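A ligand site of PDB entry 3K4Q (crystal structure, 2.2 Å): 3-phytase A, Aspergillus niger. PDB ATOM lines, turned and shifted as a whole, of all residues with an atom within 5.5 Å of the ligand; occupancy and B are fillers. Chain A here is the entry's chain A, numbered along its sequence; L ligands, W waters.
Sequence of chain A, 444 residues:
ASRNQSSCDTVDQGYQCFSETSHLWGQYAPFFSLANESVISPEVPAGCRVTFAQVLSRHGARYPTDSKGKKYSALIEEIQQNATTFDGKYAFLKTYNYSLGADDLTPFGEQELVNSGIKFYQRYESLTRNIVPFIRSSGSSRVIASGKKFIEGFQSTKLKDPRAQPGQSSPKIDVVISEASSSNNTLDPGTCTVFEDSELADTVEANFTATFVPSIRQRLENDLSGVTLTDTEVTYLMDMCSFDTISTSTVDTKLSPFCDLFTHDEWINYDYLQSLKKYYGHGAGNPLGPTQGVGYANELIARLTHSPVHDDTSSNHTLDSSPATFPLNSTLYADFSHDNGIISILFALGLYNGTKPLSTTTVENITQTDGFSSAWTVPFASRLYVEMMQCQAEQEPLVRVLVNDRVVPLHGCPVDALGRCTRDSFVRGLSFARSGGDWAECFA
Water W3 lies within hydrogen-bond range of O22 of the ligand (2.8 Å) and NZ of Lys 277 (3.4 Å).
Water W2 lies within hydrogen-bond range of N of Thr 65 (2.8 Å), O13 of the ligand (3.0 Å) and NH1 of Arg 62 (3.1 Å).
Water W1 lies within hydrogen-bond range of OH of Tyr 28 (2.9 Å) and O13 of the ligand (3.3 Å).
NH2 of Arg 58 lies within salt-bridge range of OD2 of Asp 339.
OD1 of Asn 340 sits close to OD1 of Asp 339, 3.3 Å away.
The side-chain amide oxygen of Asn 340 lies within hydrogen-bond range of the side-chain amino group of Lys 278 (2.6 Å).
NE2 of His 338 is in hydrogen-bond range of OE2 of Glu 179.
NE of Arg 142 sits at hydrogen-bond distance from NE2 of His 59 (3.4 Å).
O of Gln 27 sits at hydrogen-bond distance from NH1 of Arg 58 (2.6 Å).
The backbone NH of His 59 is in hydrogen-bond range of the backbone carbonyl oxygen of Ser 337, 3.2 Å away.
OG1 of Thr 65 sits at hydrogen-bond distance from N of Lys 68 (3.4 Å).
The backbone NH (N) of Asp 339 lies within hydrogen-bond range of an oxygen (O11) of the ligand (2.8 Å).
OD2 of Asp 339 lies close to O17 of the ligand, at 2.4 Å.
The side-chain amino group of Lys 278 is in salt-bridge range of an oxygen (O17) of the ligand (2.6 Å).
A ring nitrogen (ND1) of His 338 lies within hydrogen-bond range of an oxygen (O21) of the ligand (2.7 Å).
NH2 of Arg 142 is in salt-bridge range of O4 of the ligand (2.8 Å).
An oxygen (O13) of the ligand is in salt-bridge range of the guanidinium group (NH2) of Arg 62, at 2.9 Å.
The guanidinium group (NH2) of Arg 58 lies within salt-bridge range of an oxygen (O12) of the ligand (3.0 Å).
The side-chain hydroxyl of Tyr 28 sits at hydrogen-bond distance from an oxygen (O22) of the ligand, 3.0 Å away.
A ring nitrogen (NE2) of His 59 is in hydrogen-bond range of an oxygen (O11) of the ligand (3.1 Å).
NZ of Lys 68 lies within salt-bridge range of O23 of the ligand, 3.4 Å away.
An oxygen (O20) of the ligand lies close to the side-chain carboxylate (OD2) of Asp 188 (3.4 Å).
Residues that only touch the ligand: Gln 27 (3.1 Å) and Thr 65 (3.3 Å).
Hydrophobic or aromatic side chains that line the ligand: Tyr 28, His 59 and His 338.
12 residues have an atom within 4 Å of the ligand: Gln 27, Tyr 28, Arg 58, His 59, Arg 62, Thr 65, Lys 68, Arg 142, Asp 188, Lys 278, His 338 and Asp 339.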
ATOM      1  N   GLN A  27     -14.023  27.413  30.798  1.00  0.00           N
ATOM      2  CA  GLN A  27     -12.769  26.980  30.206  1.00  0.00           C
ATOM      3  C   GLN A  27     -11.991  28.171  29.599  1.00  0.00           C
ATOM      4  O   GLN A  27     -10.852  27.996  29.104  1.00  0.00           O
ATOM      5  CB  GLN A  27     -12.974  25.852  29.159  1.00  0.00           C
ATOM      6  CG  GLN A  27     -13.541  26.290  27.771  1.00  0.00           C
ATOM      7  CD  GLN A  27     -15.019  26.719  27.821  1.00  0.00           C
ATOM      8  OE1 GLN A  27     -15.760  26.241  28.663  1.00  0.00           O
ATOM      9  NE2 GLN A  27     -15.430  27.633  26.933  1.00  0.00           N
ATOM     10  N   TYR A  28     -12.605  29.360  29.620  1.00  0.00           N
ATOM     11  CA  TYR A  28     -11.881  30.595  29.326  1.00  0.00           C
ATOM     12  C   TYR A  28     -11.372  31.321  30.586  1.00  0.00           C
ATOM     13  O   TYR A  28     -10.899  32.434  30.491  1.00  0.00           O
ATOM     14  CB  TYR A  28     -12.707  31.585  28.456  1.00  0.00           C
ATOM     15  CG  TYR A  28     -13.244  31.016  27.151  1.00  0.00           C
ATOM     16  CD1 TYR A  28     -12.499  30.046  26.410  1.00  0.00           C
ATOM     17  CD2 TYR A  28     -14.485  31.402  26.657  1.00  0.00           C
ATOM     18  CE1 TYR A  28     -12.956  29.528  25.212  1.00  0.00           C
ATOM     19  CE2 TYR A  28     -14.976  30.860  25.430  1.00  0.00           C
ATOM     20  CZ  TYR A  28     -14.227  29.924  24.736  1.00  0.00           C
ATOM     21  OH  TYR A  28     -14.689  29.440  23.550  1.00  0.00           O
ATOM     22  N   ARG A  58      -3.507  21.368  30.692  1.00  0.00           N
ATOM     23  CA  ARG A  58      -3.993  21.978  29.491  1.00  0.00           C
ATOM     24  C   ARG A  58      -2.975  23.022  29.006  1.00  0.00           C
ATOM     25  O   ARG A  58      -2.144  23.417  29.796  1.00  0.00           O
ATOM     26  CB  ARG A  58      -5.308  22.690  29.725  1.00  0.00           C
ATOM     27  CG  ARG A  58      -5.988  23.175  28.426  1.00  0.00           C
ATOM     28  CD  ARG A  58      -7.284  23.881  28.784  1.00  0.00           C
ATOM     29  NE  ARG A  58      -7.857  24.566  27.635  1.00  0.00           N
ATOM     30  CZ  ARG A  58      -8.841  25.479  27.688  1.00  0.00           C
ATOM     31  NH1 ARG A  58      -9.448  25.829  28.824  1.00  0.00           N
ATOM     32  NH2 ARG A  58      -9.195  26.068  26.577  1.00  0.00           N
ATOM     33  N   HIS A  59      -3.087  23.461  27.740  1.00  0.00           N
ATOM     34  CA  HIS A  59      -2.204  24.486  27.225  1.00  0.00           C
ATOM     35  C   HIS A  59      -2.622  25.765  27.915  1.00  0.00           C
ATOM     36  O   HIS A  59      -3.596  25.745  28.660  1.00  0.00           O
ATOM     37  CB  HIS A  59      -2.382  24.617  25.712  1.00  0.00           C
ATOM     38  CG  HIS A  59      -3.775  24.968  25.343  1.00  0.00           C
ATOM     39  ND1 HIS A  59      -4.343  26.217  25.620  1.00  0.00           N
ATOM     40  CD2 HIS A  59      -4.741  24.219  24.744  1.00  0.00           C
ATOM     41  CE1 HIS A  59      -5.608  26.187  25.231  1.00  0.00           C
ATOM     42  NE2 HIS A  59      -5.856  25.000  24.669  1.00  0.00           N
ATOM     43  N   ARG A  62      -4.843  31.474  25.477  1.00  0.00           N
ATOM     44  CA  ARG A  62      -4.581  31.622  24.067  1.00  0.00           C
ATOM     45  C   ARG A  62      -5.397  32.741  23.426  1.00  0.00           C
ATOM     46  O   ARG A  62      -6.321  33.301  24.016  1.00  0.00           O
ATOM     47  CB  ARG A  62      -4.868  30.285  23.337  1.00  0.00           C
ATOM     48  CG  ARG A  62      -6.348  29.808  23.414  1.00  0.00           C
ATOM     49  CD  ARG A  62      -6.587  28.673  22.389  1.00  0.00           C
ATOM     50  NE  ARG A  62      -7.926  28.130  22.552  1.00  0.00           N
ATOM     51  CZ  ARG A  62      -9.063  28.657  22.073  1.00  0.00           C
ATOM     52  NH1 ARG A  62      -9.069  29.782  21.380  1.00  0.00           N
ATOM     53  NH2 ARG A  62     -10.219  28.056  22.336  1.00  0.00           N
ATOM     54  N   THR A  65      -9.549  31.040  18.329  1.00  0.00           N
ATOM     55  CA  THR A  65      -9.210  30.292  17.136  1.00  0.00           C
ATOM     56  C   THR A  65      -9.473  31.240  15.957  1.00  0.00           C
ATOM     57  O   THR A  65     -10.132  32.254  16.129  1.00  0.00           O
ATOM     58  CB  THR A  65     -10.032  29.014  16.970  1.00  0.00           C
ATOM     59  OG1 THR A  65     -11.396  29.398  16.853  1.00  0.00           O
ATOM     60  CG2 THR A  65      -9.864  28.028  18.199  1.00  0.00           C
ATOM     61  N   LYS A  68     -13.232  31.745  15.235  1.00  0.00           N
ATOM     62  CA  LYS A  68     -13.965  32.568  16.185  1.00  0.00           C
ATOM     63  C   LYS A  68     -13.486  33.989  16.124  1.00  0.00           C
ATOM     64  O   LYS A  68     -14.279  34.926  16.223  1.00  0.00           O
ATOM     65  CB  LYS A  68     -13.870  32.059  17.606  1.00  0.00           C
ATOM     66  CG  LYS A  68     -14.634  30.785  17.853  1.00  0.00           C
ATOM     67  CD  LYS A  68     -16.096  31.047  18.160  1.00  0.00           C
ATOM     68  CE  LYS A  68     -16.798  29.774  18.544  1.00  0.00           C
ATOM     69  NZ  LYS A  68     -17.408  30.047  19.870  1.00  0.00           N
ATOM     70  N   ASP A 103      -5.147  31.578  17.493  1.00  0.00           N
ATOM     71  CA  ASP A 103      -4.708  30.205  17.875  1.00  0.00           C
ATOM     72  C   ASP A 103      -3.590  30.080  18.927  1.00  0.00           C
ATOM     73  O   ASP A 103      -3.658  29.229  19.820  1.00  0.00           O
ATOM     74  CB  ASP A 103      -4.355  29.371  16.629  1.00  0.00           C
ATOM     75  CG  ASP A 103      -5.568  29.165  15.688  1.00  0.00           C
ATOM     76  OD1 ASP A 103      -6.549  28.514  16.105  1.00  0.00           O
ATOM     77  OD2 ASP A 103      -5.545  29.658  14.554  1.00  0.00           O
ATOM     78  N   ARG A 142      -0.067  25.060  20.136  1.00  0.00           N
ATOM     79  CA  ARG A 142      -0.237  25.738  21.420  1.00  0.00           C
ATOM     80  C   ARG A 142       0.007  24.771  22.609  1.00  0.00           C
ATOM     81  O   ARG A 142       0.437  25.163  23.707  1.00  0.00           O
ATOM     82  CB  ARG A 142      -1.587  26.436  21.486  1.00  0.00           C
ATOM     83  CG  ARG A 142      -2.863  25.501  21.311  1.00  0.00           C
ATOM     84  CD  ARG A 142      -4.169  26.238  21.745  1.00  0.00           C
ATOM     85  NE  ARG A 142      -5.373  25.483  21.361  1.00  0.00           N
ATOM     86  CZ  ARG A 142      -5.907  25.522  20.121  1.00  0.00           C
ATOM     87  NH1 ARG A 142      -5.365  26.295  19.203  1.00  0.00           N
ATOM     88  NH2 ARG A 142      -6.995  24.798  19.833  1.00  0.00           N
ATOM     89  N   GLU A 179      -2.347  14.640  16.202  1.00  0.00           N
ATOM     90  CA  GLU A 179      -3.805  14.892  16.143  1.00  0.00           C
ATOM     91  C   GLU A 179      -4.441  14.571  14.768  1.00  0.00           C
ATOM     92  O   GLU A 179      -5.628  14.803  14.569  1.00  0.00           O
ATOM     93  CB  GLU A 179      -4.168  16.343  16.516  1.00  0.00           C
ATOM     94  CG  GLU A 179      -3.612  16.750  17.839  1.00  0.00           C
ATOM     95  CD  GLU A 179      -4.061  18.123  18.303  1.00  0.00           C
ATOM     96  OE1 GLU A 179      -4.766  18.823  17.547  1.00  0.00           O
ATOM     97  OE2 GLU A 179      -3.705  18.499  19.432  1.00  0.00           O
ATOM     98  N   ASP A 188      -6.378  13.232  23.347  1.00  0.00           N
ATOM     99  CA  ASP A 188      -7.493  13.957  22.699  1.00  0.00           C
ATOM    100  C   ASP A 188      -7.987  13.170  21.473  1.00  0.00           C
ATOM    101  O   ASP A 188      -7.663  13.525  20.336  1.00  0.00           O
ATOM    102  CB  ASP A 188      -7.117  15.381  22.272  1.00  0.00           C
ATOM    103  CG  ASP A 188      -8.355  16.236  21.865  1.00  0.00           C
ATOM    104  OD1 ASP A 188      -9.133  16.689  22.790  1.00  0.00           O
ATOM    105  OD2 ASP A 188      -8.565  16.477  20.629  1.00  0.00           O
ATOM    106  N   LYS A 277     -21.771  22.881  28.145  1.00  0.00           N
ATOM    107  CA  LYS A 277     -21.103  22.490  26.931  1.00  0.00           C
ATOM    108  C   LYS A 277     -20.091  21.359  27.184  1.00  0.00           C
ATOM    109  O   LYS A 277     -19.993  20.380  26.403  1.00  0.00           O
ATOM    110  CB  LYS A 277     -20.341  23.674  26.361  1.00  0.00           C
ATOM    111  CG  LYS A 277     -21.130  24.900  25.923  1.00  0.00           C
ATOM    112  CD  LYS A 277     -20.295  25.576  24.807  1.00  0.00           C
ATOM    113  CE  LYS A 277     -20.117  27.045  25.100  1.00  0.00           C
ATOM    114  NZ  LYS A 277     -19.211  27.822  24.140  1.00  0.00           N
ATOM    115  N   LYS A 278     -19.324  21.484  28.271  1.00  0.00           N
ATOM    116  CA  LYS A 278     -18.311  20.486  28.533  1.00  0.00           C
ATOM    117  C   LYS A 278     -18.966  19.204  29.046  1.00  0.00           C
ATOM    118  O   LYS A 278     -18.659  18.117  28.538  1.00  0.00           O
ATOM    119  CB  LYS A 278     -17.225  21.037  29.469  1.00  0.00           C
ATOM    120  CG  LYS A 278     -16.419  22.166  28.823  1.00  0.00           C
ATOM    121  CD  LYS A 278     -16.029  21.857  27.373  1.00  0.00           C
ATOM    122  CE  LYS A 278     -15.104  22.943  26.871  1.00  0.00           C
ATOM    123  NZ  LYS A 278     -14.807  22.820  25.429  1.00  0.00           N
ATOM    124  N   SER A 337      -2.307  18.780  26.866  1.00  0.00           N
ATOM    125  CA  SER A 337      -3.465  18.517  25.982  1.00  0.00           C
ATOM    126  C   SER A 337      -4.459  19.641  26.006  1.00  0.00           C
ATOM    127  O   SER A 337      -4.163  20.726  26.551  1.00  0.00           O
ATOM    128  CB  SER A 337      -4.157  17.195  26.393  1.00  0.00           C
ATOM    129  OG  SER A 337      -4.934  16.737  25.317  1.00  0.00           O
ATOM    130  N   HIS A 338      -5.635  19.361  25.431  1.00  0.00           N
ATOM    131  CA  HIS A 338      -6.740  20.319  25.240  1.00  0.00           C
ATOM    132  C   HIS A 338      -7.783  20.057  26.325  1.00  0.00           C
ATOM    133  O   HIS A 338      -7.800  18.984  26.912  1.00  0.00           O
ATOM    134  CB  HIS A 338      -7.415  20.115  23.847  1.00  0.00           C
ATOM    135  CG  HIS A 338      -6.472  20.249  22.698  1.00  0.00           C
ATOM    136  ND1 HIS A 338      -6.233  21.467  22.079  1.00  0.00           N
ATOM    137  CD2 HIS A 338      -5.720  19.337  22.037  1.00  0.00           C
ATOM    138  CE1 HIS A 338      -5.369  21.289  21.085  1.00  0.00           C
ATOM    139  NE2 HIS A 338      -5.059  20.003  21.028  1.00  0.00           N
ATOM    140  N   ASP A 339      -8.656  21.033  26.563  1.00  0.00           N
ATOM    141  CA  ASP A 339      -9.691  20.880  27.605  1.00  0.00           C
ATOM    142  C   ASP A 339     -10.674  19.690  27.357  1.00  0.00           C
ATOM    143  O   ASP A 339     -11.068  18.993  28.275  1.00  0.00           O
ATOM    144  CB  ASP A 339     -10.453  22.189  27.725  1.00  0.00           C
ATOM    145  CG  ASP A 339     -11.074  22.619  26.420  1.00  0.00           C
ATOM    146  OD1 ASP A 339     -11.088  21.861  25.433  1.00  0.00           O
ATOM    147  OD2 ASP A 339     -11.496  23.757  26.313  1.00  0.00           O
ATOM    148  N   ASN A 340     -11.040  19.450  26.103  1.00  0.00           N
ATOM    149  CA  ASN A 340     -12.076  18.492  25.801  1.00  0.00           C
ATOM    150  C   ASN A 340     -11.604  17.099  26.150  1.00  0.00           C
ATOM    151  O   ASN A 340     -12.354  16.318  26.706  1.00  0.00           O
ATOM    152  CB  ASN A 340     -12.522  18.548  24.303  1.00  0.00           C
ATOM    153  CG  ASN A 340     -13.378  19.780  23.951  1.00  0.00           C
ATOM    154  OD1 ASN A 340     -13.973  20.482  24.821  1.00  0.00           O
ATOM    155  ND2 ASN A 340     -13.456  20.069  22.634  1.00  0.00           N
ATOM    156  N   PHE A 380      -7.917  27.665  31.479  1.00  0.00           N
ATOM    157  CA  PHE A 380      -6.627  27.827  30.812  1.00  0.00           C
ATOM    158  C   PHE A 380      -5.531  27.412  31.810  1.00  0.00           C
ATOM    159  O   PHE A 380      -5.576  27.831  32.979  1.00  0.00           O
ATOM    160  CB  PHE A 380      -6.372  29.278  30.389  1.00  0.00           C
ATOM    161  CG  PHE A 380      -7.182  29.722  29.207  1.00  0.00           C
ATOM    162  CD1 PHE A 380      -7.186  28.957  28.011  1.00  0.00           C
ATOM    163  CD2 PHE A 380      -7.919  30.917  29.267  1.00  0.00           C
ATOM    164  CE1 PHE A 380      -7.927  29.368  26.900  1.00  0.00           C
ATOM    165  CE2 PHE A 380      -8.613  31.356  28.156  1.00  0.00           C
ATOM    166  CZ  PHE A 380      -8.645  30.563  26.975  1.00  0.00           C
HETATM  167  C1  LIG L   1     -10.907  23.901  19.457  1.00  0.00           C
HETATM  168  O1  LIG L   1     -10.588  23.234  18.313  1.00  0.00           O
HETATM  169  S1  LIG L   1      -9.829  24.009  17.250  1.00  0.00           S
HETATM  170  C2  LIG L   1     -10.101  23.338  20.612  1.00  0.00           C
HETATM  171  O2  LIG L   1     -10.806  24.656  16.361  1.00  0.00           O
HETATM  172  S2  LIG L   1      -9.318  20.907  20.054  1.00  0.00           S
HETATM  173  C3  LIG L   1     -10.513  24.065  21.868  1.00  0.00           C
HETATM  174  O3  LIG L   1      -9.179  22.832  16.669  1.00  0.00           O
HETATM  175  S3  LIG L   1      -8.707  23.900  23.503  1.00  0.00           S
HETATM  176  C4  LIG L   1     -11.932  24.593  21.949  1.00  0.00           C
HETATM  177  O4  LIG L   1      -8.768  24.941  17.668  1.00  0.00           O
HETATM  178  S4  LIG L   1     -12.516  25.734  24.086  1.00  0.00           S
HETATM  179  C5  LIG L   1     -12.425  25.167  20.610  1.00  0.00           C
HETATM  180  S5  LIG L   1     -13.877  27.272  20.412  1.00  0.00           S
HETATM  181  C6  LIG L   1     -12.405  24.011  19.618  1.00  0.00           C
HETATM  182  S6  LIG L   1     -14.172  23.852  17.666  1.00  0.00           S
HETATM  183  O5  LIG L   1     -10.136  21.928  20.830  1.00  0.00           O
HETATM  184  O6  LIG L   1     -10.063  23.373  23.050  1.00  0.00           O
HETATM  185  O7  LIG L   1     -11.707  25.665  22.813  1.00  0.00           O
HETATM  186  O8  LIG L   1     -13.701  25.783  20.684  1.00  0.00           O
HETATM  187  O9  LIG L   1     -12.974  24.471  18.403  1.00  0.00           O
HETATM  188  O10 LIG L   1     -10.142  20.476  18.899  1.00  0.00           O
HETATM  189  O11 LIG L   1      -8.403  23.238  24.783  1.00  0.00           O
HETATM  190  O12 LIG L   1     -11.829  26.416  25.186  1.00  0.00           O
HETATM  191  O13 LIG L   1     -12.856  28.031  21.150  1.00  0.00           O
HETATM  192  O14 LIG L   1     -15.319  23.899  18.606  1.00  0.00           O
HETATM  193  O15 LIG L   1      -8.080  21.433  19.496  1.00  0.00           O
HETATM  194  O16 LIG L   1      -8.826  25.391  23.577  1.00  0.00           O
HETATM  195  O17 LIG L   1     -12.949  24.409  24.505  1.00  0.00           O
HETATM  196  O18 LIG L   1     -13.739  27.532  18.972  1.00  0.00           O
HETATM  197  O19 LIG L   1     -13.890  22.474  17.236  1.00  0.00           O
HETATM  198  O20 LIG L   1      -9.172  19.760  20.950  1.00  0.00           O
HETATM  199  O21 LIG L   1      -7.662  23.707  22.503  1.00  0.00           O
HETATM  200  O22 LIG L   1     -13.602  26.641  23.605  1.00  0.00           O
HETATM  201  O23 LIG L   1     -15.210  27.685  20.877  1.00  0.00           O
HETATM  202  O24 LIG L   1     -14.389  24.707  16.484  1.00  0.00           O
HETATM  203  O   HOH W   1     -13.614  31.271  21.504  1.00  0.00           O
HETATM  204  O   HOH W   2     -11.710  30.520  19.954  1.00  0.00           O
HETATM  205  O   HOH W   3     -16.336  25.973  23.873  1.00  0.00           O
